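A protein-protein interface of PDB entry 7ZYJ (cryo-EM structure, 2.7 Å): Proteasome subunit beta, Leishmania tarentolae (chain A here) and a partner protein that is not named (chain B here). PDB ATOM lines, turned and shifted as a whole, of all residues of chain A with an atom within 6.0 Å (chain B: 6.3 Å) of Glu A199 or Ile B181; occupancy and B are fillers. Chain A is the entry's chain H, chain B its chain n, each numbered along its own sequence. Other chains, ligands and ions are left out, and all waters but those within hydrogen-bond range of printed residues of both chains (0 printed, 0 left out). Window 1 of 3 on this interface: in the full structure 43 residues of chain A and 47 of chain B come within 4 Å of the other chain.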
ATOM      1  N   SER A 165      19.227  12.710   9.334  1.00  0.00           N
ATOM      2  CA  SER A 165      19.653  13.209  10.635  1.00  0.00           C
ATOM      3  C   SER A 165      20.697  14.307  10.491  1.00  0.00           C
ATOM      4  O   SER A 165      20.774  15.202  11.339  1.00  0.00           O
ATOM      5  CB  SER A 165      20.194  12.063  11.488  1.00  0.00           C
ATOM      6  OG  SER A 165      19.143  11.217  11.918  1.00  0.00           O
ATOM      7  N   TRP A 191       8.688   9.952  11.783  1.00  0.00           N
ATOM      8  CA  TRP A 191       9.938  10.396  12.388  1.00  0.00           C
ATOM      9  C   TRP A 191      10.065   9.935  13.834  1.00  0.00           C
ATOM     10  O   TRP A 191      11.166   9.583  14.273  1.00  0.00           O
ATOM     11  CB  TRP A 191      10.061  11.916  12.314  1.00  0.00           C
ATOM     12  CG  TRP A 191      11.353  12.402  12.883  1.00  0.00           C
ATOM     13  CD1 TRP A 191      12.548  12.495  12.236  1.00  0.00           C
ATOM     14  CD2 TRP A 191      11.593  12.819  14.232  1.00  0.00           C
ATOM     15  NE1 TRP A 191      13.514  12.963  13.091  1.00  0.00           N
ATOM     16  CE2 TRP A 191      12.953  13.169  14.323  1.00  0.00           C
ATOM     17  CE3 TRP A 191      10.788  12.937  15.367  1.00  0.00           C
ATOM     18  CZ2 TRP A 191      13.525  13.632  15.505  1.00  0.00           C
ATOM     19  CZ3 TRP A 191      11.357  13.396  16.537  1.00  0.00           C
ATOM     20  CH2 TRP A 191      12.712  13.736  16.597  1.00  0.00           C
ATOM     21  N   CYS A 197      17.962   8.848  15.039  1.00  0.00           N
ATOM     22  CA  CYS A 197      18.040  10.301  15.032  1.00  0.00           C
ATOM     23  C   CYS A 197      18.986  10.712  16.150  1.00  0.00           C
ATOM     24  O   CYS A 197      19.170   9.973  17.121  1.00  0.00           O
ATOM     25  CB  CYS A 197      16.665  10.955  15.210  1.00  0.00           C
ATOM     26  SG  CYS A 197      15.903  10.683  16.816  1.00  0.00           S
ATOM     27  N   MET A 198      19.592  11.893  16.004  1.00  0.00           N
ATOM     28  CA  MET A 198      20.553  12.341  17.006  1.00  0.00           C
ATOM     29  C   MET A 198      19.887  12.702  18.327  1.00  0.00           C
ATOM     30  O   MET A 198      20.562  12.715  19.362  1.00  0.00           O
ATOM     31  CB  MET A 198      21.351  13.541  16.498  1.00  0.00           C
ATOM     32  CG  MET A 198      22.221  13.257  15.289  1.00  0.00           C
ATOM     33  SD  MET A 198      23.134  14.722  14.776  1.00  0.00           S
ATOM     34  CE  MET A 198      21.802  15.785  14.239  1.00  0.00           C
ATOM     35  N   GLU A 199      18.587  13.000  18.317  1.00  0.00           N
ATOM     36  CA  GLU A 199      17.900  13.358  19.552  1.00  0.00           C
ATOM     37  C   GLU A 199      17.832  12.185  20.522  1.00  0.00           C
ATOM     38  O   GLU A 199      17.917  12.385  21.738  1.00  0.00           O
ATOM     39  CB  GLU A 199      16.496  13.873  19.239  1.00  0.00           C
ATOM     40  CG  GLU A 199      16.466  15.212  18.524  1.00  0.00           C
ATOM     41  CD  GLU A 199      16.499  15.075  17.014  1.00  0.00           C
ATOM     42  OE1 GLU A 199      17.089  14.096  16.513  1.00  0.00           O
ATOM     43  OE2 GLU A 199      15.930  15.947  16.325  1.00  0.00           O
ATOM     44  N   LYS A 200      17.674  10.966  20.012  1.00  0.00           N
ATOM     45  CA  LYS A 200      17.623   9.772  20.843  1.00  0.00           C
ATOM     46  C   LYS A 200      18.977   9.094  20.994  1.00  0.00           C
ATOM     47  O   LYS A 200      19.074   8.089  21.704  1.00  0.00           O
ATOM     48  CB  LYS A 200      16.613   8.771  20.274  1.00  0.00           C
ATOM     49  CG  LYS A 200      15.253   9.362  19.952  1.00  0.00           C
ATOM     50  CD  LYS A 200      14.597   9.968  21.174  1.00  0.00           C
ATOM     51  CE  LYS A 200      13.320  10.695  20.792  1.00  0.00           C
ATOM     52  NZ  LYS A 200      12.483   9.885  19.865  1.00  0.00           N
ATOM     53  N   ASP A 201      20.016   9.611  20.349  1.00  0.00           N
ATOM     54  CA  ASP A 201      21.331   8.989  20.417  1.00  0.00           C
ATOM     55  C   ASP A 201      21.965   9.278  21.772  1.00  0.00           C
ATOM     56  O   ASP A 201      22.143  10.451  22.121  1.00  0.00           O
ATOM     57  CB  ASP A 201      22.217   9.510  19.291  1.00  0.00           C
ATOM     58  CG  ASP A 201      23.415   8.620  19.027  1.00  0.00           C
ATOM     59  OD1 ASP A 201      23.632   7.656  19.787  1.00  0.00           O
ATOM     60  OD2 ASP A 201      24.141   8.881  18.046  1.00  0.00           O
ATOM     61  N   VAL A 205      23.760  13.131  24.192  1.00  0.00           N
ATOM     62  CA  VAL A 205      22.926  13.597  25.295  1.00  0.00           C
ATOM     63  C   VAL A 205      23.629  14.677  26.108  1.00  0.00           C
ATOM     64  O   VAL A 205      23.019  15.689  26.463  1.00  0.00           O
ATOM     65  CB  VAL A 205      22.517  12.402  26.180  1.00  0.00           C
ATOM     66  CG1 VAL A 205      22.023  12.882  27.533  1.00  0.00           C
ATOM     67  CG2 VAL A 205      21.448  11.580  25.487  1.00  0.00           C
ATOM     68  N   ASP B  21      16.307  25.788  20.366  1.00  0.00           N
ATOM     69  CA  ASP B  21      16.841  24.453  20.151  1.00  0.00           C
ATOM     70  C   ASP B  21      18.345  24.423  20.414  1.00  0.00           C
ATOM     71  O   ASP B  21      19.035  25.441  20.360  1.00  0.00           O
ATOM     72  CB  ASP B  21      16.511  23.953  18.738  1.00  0.00           C
ATOM     73  CG  ASP B  21      17.319  24.644  17.645  1.00  0.00           C
ATOM     74  OD1 ASP B  21      17.976  25.672  17.904  1.00  0.00           O
ATOM     75  OD2 ASP B  21      17.297  24.140  16.503  1.00  0.00           O
ATOM     76  N   THR B  22      18.840  23.236  20.740  1.00  0.00           N
ATOM     77  CA  THR B  22      20.254  23.048  21.067  1.00  0.00           C
ATOM     78  C   THR B  22      21.033  22.544  19.854  1.00  0.00           C
ATOM     79  O   THR B  22      21.664  21.494  19.887  1.00  0.00           O
ATOM     80  CB  THR B  22      20.395  22.091  22.248  1.00  0.00           C
ATOM     81  OG1 THR B  22      20.299  20.739  21.783  1.00  0.00           O
ATOM     82  CG2 THR B  22      19.304  22.344  23.272  1.00  0.00           C
ATOM     83  N   LEU B  23      20.996  23.312  18.767  1.00  0.00           N
ATOM     84  CA  LEU B  23      21.637  22.901  17.527  1.00  0.00           C
ATOM     85  C   LEU B  23      22.419  24.050  16.909  1.00  0.00           C
ATOM     86  O   LEU B  23      21.930  25.182  16.845  1.00  0.00           O
ATOM     87  CB  LEU B  23      20.605  22.383  16.517  1.00  0.00           C
ATOM     88  CG  LEU B  23      21.121  22.084  15.107  1.00  0.00           C
ATOM     89  CD1 LEU B  23      21.767  20.711  15.047  1.00  0.00           C
ATOM     90  CD2 LEU B  23      20.004  22.202  14.086  1.00  0.00           C
ATOM     91  N   ALA B  30      23.513  19.808   9.789  1.00  0.00           N
ATOM     92  CA  ALA B  30      23.250  19.839  11.225  1.00  0.00           C
ATOM     93  C   ALA B  30      24.508  19.365  11.937  1.00  0.00           C
ATOM     94  O   ALA B  30      24.711  18.166  12.137  1.00  0.00           O
ATOM     95  CB  ALA B  30      22.049  18.968  11.572  1.00  0.00           C
ATOM     96  N   TRP B  32      26.233  20.272  15.118  1.00  0.00           N
ATOM     97  CA  TRP B  32      26.343  19.954  16.539  1.00  0.00           C
ATOM     98  C   TRP B  32      24.966  19.988  17.187  1.00  0.00           C
ATOM     99  O   TRP B  32      24.356  21.073  17.283  1.00  0.00           O
ATOM    100  CB  TRP B  32      27.295  20.921  17.240  1.00  0.00           C
ATOM    101  CG  TRP B  32      28.688  20.870  16.716  1.00  0.00           C
ATOM    102  CD1 TRP B  32      29.475  19.766  16.585  1.00  0.00           C
ATOM    103  CD2 TRP B  32      29.468  21.976  16.251  1.00  0.00           C
ATOM    104  NE1 TRP B  32      30.696  20.114  16.065  1.00  0.00           N
ATOM    105  CE2 TRP B  32      30.717  21.466  15.853  1.00  0.00           C
ATOM    106  CE3 TRP B  32      29.230  23.348  16.134  1.00  0.00           C
ATOM    107  CZ2 TRP B  32      31.725  22.280  15.346  1.00  0.00           C
ATOM    108  CZ3 TRP B  32      30.232  24.152  15.629  1.00  0.00           C
ATOM    109  CH2 TRP B  32      31.464  23.616  15.242  1.00  0.00           C
ATOM    110  N   PRO B  33      24.442  18.855  17.649  1.00  0.00           N
ATOM    111  CA  PRO B  33      23.112  18.827  18.275  1.00  0.00           C
ATOM    112  C   PRO B  33      23.103  18.941  19.793  1.00  0.00           C
ATOM    113  O   PRO B  33      22.042  18.747  20.393  1.00  0.00           O
ATOM    114  CB  PRO B  33      22.596  17.449  17.847  1.00  0.00           C
ATOM    115  CG  PRO B  33      23.829  16.600  17.850  1.00  0.00           C
ATOM    116  CD  PRO B  33      24.984  17.499  17.456  1.00  0.00           C
ATOM    117  N   ASN B  34      24.229  19.243  20.431  1.00  0.00           N
ATOM    118  CA  ASN B  34      24.326  19.289  21.889  1.00  0.00           C
ATOM    119  C   ASN B  34      24.980  20.589  22.346  1.00  0.00           C
ATOM    120  O   ASN B  34      25.890  20.600  23.176  1.00  0.00           O
ATOM    121  CB  ASN B  34      25.091  18.076  22.411  1.00  0.00           C
ATOM    122  CG  ASN B  34      26.487  17.974  21.831  1.00  0.00           C
ATOM    123  OD1 ASN B  34      26.733  18.382  20.698  1.00  0.00           O
ATOM    124  ND2 ASN B  34      27.411  17.427  22.611  1.00  0.00           N
ATOM    125  N   PHE B 174       9.663  22.766  14.665  1.00  0.00           N
ATOM    126  CA  PHE B 174      10.278  21.513  14.247  1.00  0.00           C
ATOM    127  C   PHE B 174       9.599  20.950  13.006  1.00  0.00           C
ATOM    128  O   PHE B 174      10.265  20.353  12.154  1.00  0.00           O
ATOM    129  CB  PHE B 174      10.234  20.495  15.383  1.00  0.00           C
ATOM    130  CG  PHE B 174      10.787  19.152  15.010  1.00  0.00           C
ATOM    131  CD1 PHE B 174      12.100  19.020  14.595  1.00  0.00           C
ATOM    132  CD2 PHE B 174       9.991  18.022  15.065  1.00  0.00           C
ATOM    133  CE1 PHE B 174      12.611  17.786  14.248  1.00  0.00           C
ATOM    134  CE2 PHE B 174      10.496  16.785  14.717  1.00  0.00           C
ATOM    135  CZ  PHE B 174      11.807  16.668  14.309  1.00  0.00           C
ATOM    136  N   GLU B 177      10.601  24.115  10.053  1.00  0.00           N
ATOM    137  CA  GLU B 177      11.927  24.695   9.873  1.00  0.00           C
ATOM    138  C   GLU B 177      12.910  23.598   9.491  1.00  0.00           C
ATOM    139  O   GLU B 177      12.980  22.562  10.159  1.00  0.00           O
ATOM    140  CB  GLU B 177      12.396  25.419  11.137  1.00  0.00           C
ATOM    141  CG  GLU B 177      13.614  26.299  10.925  1.00  0.00           C
ATOM    142  CD  GLU B 177      14.276  26.703  12.227  1.00  0.00           C
ATOM    143  OE1 GLU B 177      13.763  26.321  13.300  1.00  0.00           O
ATOM    144  OE2 GLU B 177      15.310  27.401  12.178  1.00  0.00           O
ATOM    145  N   CYS B 178      13.662  23.830   8.414  1.00  0.00           N
ATOM    146  CA  CYS B 178      14.556  22.804   7.889  1.00  0.00           C
ATOM    147  C   CYS B 178      15.720  22.541   8.836  1.00  0.00           C
ATOM    148  O   CYS B 178      16.021  21.388   9.166  1.00  0.00           O
ATOM    149  CB  CYS B 178      15.070  23.219   6.510  1.00  0.00           C
ATOM    150  SG  CYS B 178      13.803  23.256   5.236  1.00  0.00           S
ATOM    151  N   ARG B 179      16.391  23.601   9.284  1.00  0.00           N
ATOM    152  CA  ARG B 179      17.578  23.465  10.125  1.00  0.00           C
ATOM    153  C   ARG B 179      17.151  23.532  11.587  1.00  0.00           C
ATOM    154  O   ARG B 179      17.404  24.500  12.307  1.00  0.00           O
ATOM    155  CB  ARG B 179      18.606  24.533   9.778  1.00  0.00           C
ATOM    156  CG  ARG B 179      19.311  24.292   8.456  1.00  0.00           C
ATOM    157  CD  ARG B 179      19.721  25.593   7.794  1.00  0.00           C
ATOM    158  NE  ARG B 179      19.773  25.466   6.343  1.00  0.00           N
ATOM    159  CZ  ARG B 179      20.351  26.343   5.533  1.00  0.00           C
ATOM    160  NH1 ARG B 179      20.941  27.430   6.001  1.00  0.00           N
ATOM    161  NH2 ARG B 179      20.337  26.121   4.222  1.00  0.00           N
ATOM    162  N   ALA B 180      16.486  22.468  12.028  1.00  0.00           N
ATOM    163  CA  ALA B 180      16.025  22.366  13.403  1.00  0.00           C
ATOM    164  C   ALA B 180      16.074  20.910  13.836  1.00  0.00           C
ATOM    165  O   ALA B 180      16.071  19.995  13.008  1.00  0.00           O
ATOM    166  CB  ALA B 180      14.608  22.927  13.564  1.00  0.00           C
ATOM    167  N   ILE B 181      16.126  20.706  15.151  1.00  0.00           N
ATOM    168  CA  ILE B 181      16.075  19.378  15.744  1.00  0.00           C
ATOM    169  C   ILE B 181      15.042  19.394  16.860  1.00  0.00           C
ATOM    170  O   ILE B 181      14.682  20.445  17.392  1.00  0.00           O
ATOM    171  CB  ILE B 181      17.445  18.914  16.286  1.00  0.00           C
ATOM    172  CG1 ILE B 181      17.956  19.884  17.351  1.00  0.00           C
ATOM    173  CG2 ILE B 181      18.451  18.773  15.158  1.00  0.00           C
ATOM    174  CD1 ILE B 181      19.148  19.368  18.119  1.00  0.00           C
ATOM    175  N   ASN B 182      14.562  18.204  17.209  1.00  0.00           N
ATOM    176  CA  ASN B 182      13.580  18.059  18.283  1.00  0.00           C
ATOM    177  C   ASN B 182      14.288  17.914  19.632  1.00  0.00           C
ATOM    178  O   ASN B 182      14.235  16.884  20.300  1.00  0.00           O
ATOM    179  CB  ASN B 182      12.660  16.878  18.003  1.00  0.00           C
ATOM    180  CG  ASN B 182      11.398  16.910  18.839  1.00  0.00           C
ATOM    181  OD1 ASN B 182      11.106  17.904  19.501  1.00  0.00           O
ATOM    182  ND2 ASN B 182      10.641  15.822  18.811  1.00  0.00           N
ATOM    183  N   LYS B 183      14.973  18.989  20.016  1.00  0.00           N
ATOM    184  CA  LYS B 183      15.659  19.056  21.305  1.00  0.00           C
ATOM    185  C   LYS B 183      15.786  20.527  21.670  1.00  0.00           C
ATOM    186  O   LYS B 183      16.520  21.266  21.009  1.00  0.00           O
ATOM    187  CB  LYS B 183      17.024  18.378  21.244  1.00  0.00           C
ATOM    188  CG  LYS B 183      17.579  17.993  22.603  1.00  0.00           C
ATOM    189  CD  LYS B 183      18.413  16.728  22.519  1.00  0.00           C
ATOM    190  CE  LYS B 183      19.792  17.011  21.950  1.00  0.00           C
ATOM    191  NZ  LYS B 183      20.631  15.784  21.894  1.00  0.00           N
ATOM    192  N   PHE B 184      15.078  20.947  22.712  1.00  0.00           N
ATOM    193  CA  PHE B 184      14.971  22.353  23.061  1.00  0.00           C
ATOM    194  C   PHE B 184      15.310  22.569  24.528  1.00  0.00           C
ATOM    195  O   PHE B 184      15.207  21.660  25.356  1.00  0.00           O
ATOM    196  CB  PHE B 184      13.563  22.888  22.778  1.00  0.00           C
ATOM    197  CG  PHE B 184      13.006  22.459  21.454  1.00  0.00           C
ATOM    198  CD1 PHE B 184      13.349  23.127  20.293  1.00  0.00           C
ATOM    199  CD2 PHE B 184      12.140  21.382  21.371  1.00  0.00           C
ATOM    200  CE1 PHE B 184      12.836  22.731  19.076  1.00  0.00           C
ATOM    201  CE2 PHE B 184      11.625  20.983  20.157  1.00  0.00           C
ATOM    202  CZ  PHE B 184      11.975  21.657  19.008  1.00  0.00           C
ATOM    203  N   ASP B 201      12.283  17.216  24.540  1.00  0.00           N
ATOM    204  CA  ASP B 201      11.689  17.131  23.217  1.00  0.00           C
ATOM    205  C   ASP B 201      10.172  17.165  23.335  1.00  0.00           C
ATOM    206  O   ASP B 201       9.600  16.822  24.372  1.00  0.00           O
ATOM    207  CB  ASP B 201      12.137  15.862  22.474  1.00  0.00           C
ATOM    208  CG  ASP B 201      11.983  14.606  23.310  1.00  0.00           C
ATOM    209  OD1 ASP B 201      10.864  14.331  23.790  1.00  0.00           O
ATOM    210  OD2 ASP B 201      12.990  13.888  23.489  1.00  0.00           O
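Of the 17 printed residues of chain B, 6 touch a printed residue of chain A.
Printed residues of chain B that touch a printed residue of chain A: Ala B30, Pro B33, Phe B174, Ile B181, Asn B182 and Lys B183.
Among the printed residues, 7 pairs touch across the chains.
The side-chain carboxylate (OE2) of Glu A199 sits at hydrogen-bond distance from the backbone NH (N) of Asn B182 (2.8 Å).
Among the printed residues, merely in contact across the chains: Ser A165 with Ala B30 (3.98 Å), Trp A191 with Phe B174 (3.7 Å), Trp A191 with Asn B182 (3.4 Å), Met A198 with Pro B33 (3.7 Å), Met A198 with Lys B183 (3.98 Å) and Glu A199 with Ile B181 (3.3 Å).
The side-chain hydroxyl (OG1) of Thr B22 is in hydrogen-bond range of the backbone carbonyl oxygen (O) of Pro B33 (3.0 Å).
The backbone carbonyl oxygen (O) of Lys B183 sits at hydrogen-bond distance from the backbone NH (N) of Thr B22, at 3.1 Å.
SG of Cys A197 lies close to OE1 of Glu A199 (3.6 Å).
Of the printed residues of chain B, Ser A165 touches Ala B30 (3.98 Å).
Of the printed residues of chain B, Trp A191 touches Phe B174 (3.7 Å) and Asn B182 (3.4 Å).
Glu A199 touches just these residues of chain B: Ile B181 and Asn B182.
Printed residues of chain A within 4 Å of Ala B30: Ser A165.
Of the printed residues of chain A, Phe B174 touches Trp A191 (3.7 Å).
Of chain A, only Glu A199 comes within 4 Å of Ile B181.
Printed residues of chain A within 4 Å of Asn B182: Trp A191 and Glu A199.
The nearest residue of chain B that does not touch Glu A199 is Lys B183 (4.2 Å).
The nearest residue of chain A that does not touch Ile B181 is Met A198 (4.6 Å).
The nearest printed residue of chain A that does not touch Lys B183 is Glu A199 (4.2 Å).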
